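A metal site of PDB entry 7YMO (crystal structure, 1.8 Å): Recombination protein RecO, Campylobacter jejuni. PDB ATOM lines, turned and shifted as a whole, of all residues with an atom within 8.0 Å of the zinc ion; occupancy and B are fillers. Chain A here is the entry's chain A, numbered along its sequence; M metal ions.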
ATOM      1  N   PHE A 146      31.364   6.120 -14.799  1.00  0.00           N
ATOM      2  CA  PHE A 146      30.043   5.655 -15.205  1.00  0.00           C
ATOM      3  C   PHE A 146      29.154   5.589 -13.965  1.00  0.00           C
ATOM      4  O   PHE A 146      29.562   5.043 -12.938  1.00  0.00           O
ATOM      5  CB  PHE A 146      30.123   4.290 -15.887  1.00  0.00           C
ATOM      6  CG  PHE A 146      30.729   4.338 -17.263  1.00  0.00           C
ATOM      7  CD1 PHE A 146      29.985   4.749 -18.351  1.00  0.00           C
ATOM      8  CD2 PHE A 146      32.060   3.991 -17.456  1.00  0.00           C
ATOM      9  CE1 PHE A 146      30.548   4.797 -19.620  1.00  0.00           C
ATOM     10  CE2 PHE A 146      32.628   4.046 -18.713  1.00  0.00           C
ATOM     11  CZ  PHE A 146      31.876   4.445 -19.800  1.00  0.00           C
ATOM     12  N   CYS A 147      27.949   6.145 -14.082  1.00  0.00           N
ATOM     13  CA  CYS A 147      27.071   6.276 -12.911  1.00  0.00           C
ATOM     14  C   CYS A 147      26.635   4.907 -12.405  1.00  0.00           C
ATOM     15  O   CYS A 147      26.209   4.047 -13.169  1.00  0.00           O
ATOM     16  CB  CYS A 147      25.836   7.117 -13.279  1.00  0.00           C
ATOM     17  SG  CYS A 147      24.689   7.413 -11.900  1.00  0.00           S
ATOM     18  N   PHE A 148      26.746   4.717 -11.087  1.00  0.00           N
ATOM     19  CA  PHE A 148      26.283   3.475 -10.469  1.00  0.00           C
ATOM     20  C   PHE A 148      24.801   3.243 -10.695  1.00  0.00           C
ATOM     21  O   PHE A 148      24.360   2.090 -10.709  1.00  0.00           O
ATOM     22  CB  PHE A 148      26.576   3.512  -8.962  1.00  0.00           C
ATOM     23  CG  PHE A 148      25.496   4.199  -8.159  1.00  0.00           C
ATOM     24  CD1 PHE A 148      25.401   5.580  -8.146  1.00  0.00           C
ATOM     25  CD2 PHE A 148      24.572   3.455  -7.453  1.00  0.00           C
ATOM     26  CE1 PHE A 148      24.392   6.211  -7.412  1.00  0.00           C
ATOM     27  CE2 PHE A 148      23.563   4.077  -6.722  1.00  0.00           C
ATOM     28  CZ  PHE A 148      23.476   5.460  -6.714  1.00  0.00           C
ATOM     29  N   ALA A 149      24.024   4.317 -10.876  1.00  0.00           N
ATOM     30  CA  ALA A 149      22.568   4.236 -10.930  1.00  0.00           C
ATOM     31  C   ALA A 149      22.028   4.041 -12.341  1.00  0.00           C
ATOM     32  O   ALA A 149      21.220   3.146 -12.581  1.00  0.00           O
ATOM     33  CB  ALA A 149      21.941   5.486 -10.307  1.00  0.00           C
ATOM     34  N   CYS A 150      22.455   4.880 -13.286  1.00  0.00           N
ATOM     35  CA  CYS A 150      21.914   4.857 -14.639  1.00  0.00           C
ATOM     36  C   CYS A 150      22.891   4.293 -15.671  1.00  0.00           C
ATOM     37  O   CYS A 150      22.547   4.219 -16.862  1.00  0.00           O
ATOM     38  CB  CYS A 150      21.483   6.257 -15.068  1.00  0.00           C
ATOM     39  SG  CYS A 150      22.865   7.366 -15.428  1.00  0.00           S
ATOM     40  N   ASP A 151      24.096   3.932 -15.246  1.00  0.00           N
ATOM     41  CA  ASP A 151      25.152   3.335 -16.066  1.00  0.00           C
ATOM     42  C   ASP A 151      25.589   4.215 -17.232  1.00  0.00           C
ATOM     43  O   ASP A 151      26.132   3.707 -18.219  1.00  0.00           O
ATOM     44  CB  ASP A 151      24.750   1.945 -16.581  1.00  0.00           C
ATOM     45  CG  ASP A 151      25.956   1.078 -16.887  1.00  0.00           C
ATOM     46  OD1 ASP A 151      27.083   1.477 -16.532  1.00  0.00           O
ATOM     47  OD2 ASP A 151      25.771  -0.014 -17.480  1.00  0.00           O
ATOM     48  N   GLU A 152      25.385   5.513 -17.158  1.00  0.00           N
ATOM     49  CA  GLU A 152      25.822   6.407 -18.219  1.00  0.00           C
ATOM     50  C   GLU A 152      27.085   7.149 -17.818  1.00  0.00           C
ATOM     51  O   GLU A 152      27.383   7.321 -16.637  1.00  0.00           O
ATOM     52  CB  GLU A 152      24.724   7.408 -18.566  1.00  0.00           C
ATOM     53  CG  GLU A 152      23.527   6.761 -19.210  1.00  0.00           C
ATOM     54  CD  GLU A 152      22.521   7.782 -19.653  1.00  0.00           C
ATOM     55  OE1 GLU A 152      22.764   8.992 -19.480  1.00  0.00           O
ATOM     56  OE2 GLU A 152      21.480   7.369 -20.188  1.00  0.00           O
ATOM     57  N   LYS A 153      27.827   7.591 -18.827  1.00  0.00           N
ATOM     58  CA  LYS A 153      29.007   8.410 -18.584  1.00  0.00           C
ATOM     59  C   LYS A 153      28.639   9.671 -17.810  1.00  0.00           C
ATOM     60  O   LYS A 153      27.602  10.301 -18.072  1.00  0.00           O
ATOM     61  CB  LYS A 153      29.670   8.767 -19.921  1.00  0.00           C
ATOM     62  CG  LYS A 153      31.118   9.227 -19.823  1.00  0.00           C
ATOM     63  CD  LYS A 153      31.709   9.400 -21.223  1.00  0.00           C
ATOM     64  CE  LYS A 153      33.089   8.758 -21.334  1.00  0.00           C
ATOM     65  NZ  LYS A 153      33.333   8.194 -22.699  1.00  0.00           N
ATOM     66  N   ILE A 154      29.475  10.028 -16.845  1.00  0.00           N
ATOM     67  CA  ILE A 154      29.383  11.266 -16.083  1.00  0.00           C
ATOM     68  C   ILE A 154      30.527  12.163 -16.537  1.00  0.00           C
ATOM     69  O   ILE A 154      31.679  11.725 -16.571  1.00  0.00           O
ATOM     70  CB  ILE A 154      29.496  11.014 -14.572  1.00  0.00           C
ATOM     71  CG1 ILE A 154      28.645   9.818 -14.134  1.00  0.00           C
ATOM     72  CG2 ILE A 154      29.153  12.269 -13.779  1.00  0.00           C
ATOM     73  CD1 ILE A 154      29.220   9.113 -12.886  1.00  0.00           C
ATOM     74  N   PRO A 166      31.091   6.574  -8.195  1.00  0.00           N
ATOM     75  CA  PRO A 166      30.649   7.742  -8.948  1.00  0.00           C
ATOM     76  C   PRO A 166      29.172   7.727  -9.321  1.00  0.00           C
ATOM     77  O   PRO A 166      28.563   6.678  -9.524  1.00  0.00           O
ATOM     78  CB  PRO A 166      31.527   7.691 -10.220  1.00  0.00           C
ATOM     79  CG  PRO A 166      31.830   6.260 -10.409  1.00  0.00           C
ATOM     80  CD  PRO A 166      31.888   5.644  -9.020  1.00  0.00           C
ATOM     81  N   SER A 167      28.601   8.937  -9.437  1.00  0.00           N
ATOM     82  CA  SER A 167      27.194   9.133  -9.736  1.00  0.00           C
ATOM     83  C   SER A 167      26.997  10.457 -10.470  1.00  0.00           C
ATOM     84  O   SER A 167      27.829  11.359 -10.385  1.00  0.00           O
ATOM     85  CB  SER A 167      26.333   9.106  -8.452  1.00  0.00           C
ATOM     86  OG  SER A 167      24.971   9.300  -8.797  1.00  0.00           O
ATOM     87  N   HIS A 168      25.887  10.568 -11.211  1.00  0.00           N
ATOM     88  CA  HIS A 168      25.367  11.883 -11.569  1.00  0.00           C
ATOM     89  C   HIS A 168      24.744  12.535 -10.351  1.00  0.00           C
ATOM     90  O   HIS A 168      24.108  11.870  -9.529  1.00  0.00           O
ATOM     91  CB  HIS A 168      24.318  11.778 -12.667  1.00  0.00           C
ATOM     92  CG  HIS A 168      24.839  11.260 -13.971  1.00  0.00           C
ATOM     93  ND1 HIS A 168      24.657   9.960 -14.382  1.00  0.00           N
ATOM     94  CD2 HIS A 168      25.545  11.874 -14.960  1.00  0.00           C
ATOM     95  CE1 HIS A 168      25.232   9.782 -15.559  1.00  0.00           C
ATOM     96  NE2 HIS A 168      25.773  10.927 -15.936  1.00  0.00           N
ATOM     97  N   SER A 169      24.905  13.854 -10.222  1.00  0.00           N
ATOM     98  CA  SER A 169      24.256  14.560  -9.120  1.00  0.00           C
ATOM     99  C   SER A 169      22.735  14.393  -9.182  1.00  0.00           C
ATOM    100  O   SER A 169      22.073  14.347  -8.134  1.00  0.00           O
ATOM    101  CB  SER A 169      24.636  16.039  -9.131  1.00  0.00           C
ATOM    102  OG  SER A 169      24.134  16.691 -10.283  1.00  0.00           O
ATOM    103  N   GLN A 170      22.168  14.287 -10.379  1.00  0.00           N
ATOM    104  CA  GLN A 170      20.723  14.052 -10.506  1.00  0.00           C
ATOM    105  C   GLN A 170      20.329  12.629 -10.136  1.00  0.00           C
ATOM    106  O   GLN A 170      19.135  12.372  -9.940  1.00  0.00           O
ATOM    107  CB  GLN A 170      20.262  14.360 -11.930  1.00  0.00           C
ATOM    108  CG  GLN A 170      20.811  15.644 -12.506  1.00  0.00           C
ATOM    109  CD  GLN A 170      21.992  15.419 -13.441  1.00  0.00           C
ATOM    110  OE1 GLN A 170      23.099  15.127 -12.987  1.00  0.00           O
ATOM    111  NE2 GLN A 170      21.754  15.542 -14.742  1.00  0.00           N
ATOM    112  N   CYS A 171      21.273  11.697 -10.050  1.00  0.00           N
ATOM    113  CA  CYS A 171      20.943  10.321  -9.711  1.00  0.00           C
ATOM    114  C   CYS A 171      21.149   9.993  -8.240  1.00  0.00           C
ATOM    115  O   CYS A 171      20.538   9.028  -7.754  1.00  0.00           O
ATOM    116  CB  CYS A 171      21.776   9.332 -10.544  1.00  0.00           C
ATOM    117  SG  CYS A 171      21.514   9.394 -12.369  1.00  0.00           S
ATOM    118  N   ALA A 172      21.995  10.736  -7.533  1.00  0.00           N
ATOM    119  CA  ALA A 172      22.245  10.405  -6.132  1.00  0.00           C
ATOM    120  C   ALA A 172      22.830  11.598  -5.407  1.00  0.00           C
ATOM    121  O   ALA A 172      23.552  12.415  -5.996  1.00  0.00           O
ATOM    122  CB  ALA A 172      23.181   9.210  -6.003  1.00  0.00           C
HETATM  123 ZN    ZN M   1      23.296   8.545 -13.379  1.00  0.00          ZN
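A ring nitrogen (NE2) of His 168 is in hydrogen-bond range of the backbone carbonyl oxygen (O) of Lys 153.
The side-chain sulfur (SG) of Cys 147 sits close to the backbone NH (N) of Ala 149.
The side-chain sulfur (SG) of Cys 147 lies close to the side-chain hydroxyl (OG) of Ser 167 (3.6 Å).
The backbone NH (N) of Cys 147 is in hydrogen-bond range of the backbone carbonyl oxygen (O) of Glu 152, 2.9 Å away.
SG of Cys 150 lies close to N of Glu 152.
Within 4 Å of the zinc ion: Cys 147, Cys 150, His 168 and Cys 171.
Along chain A the residues within 4 Å of the zinc ion span positions 147 to 171.
The zinc ion is bound by a ring nitrogen (ND1) of His 168 (2.2 Å), the side-chain sulfur (SG) of Cys 171 (2.2 Å), the side-chain sulfur (SG) of Cys 147 (2.3 Å) and the side-chain sulfur (SG) of Cys 150 (2.4 Å).
The zinc ion has four donor atoms within binding distance.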
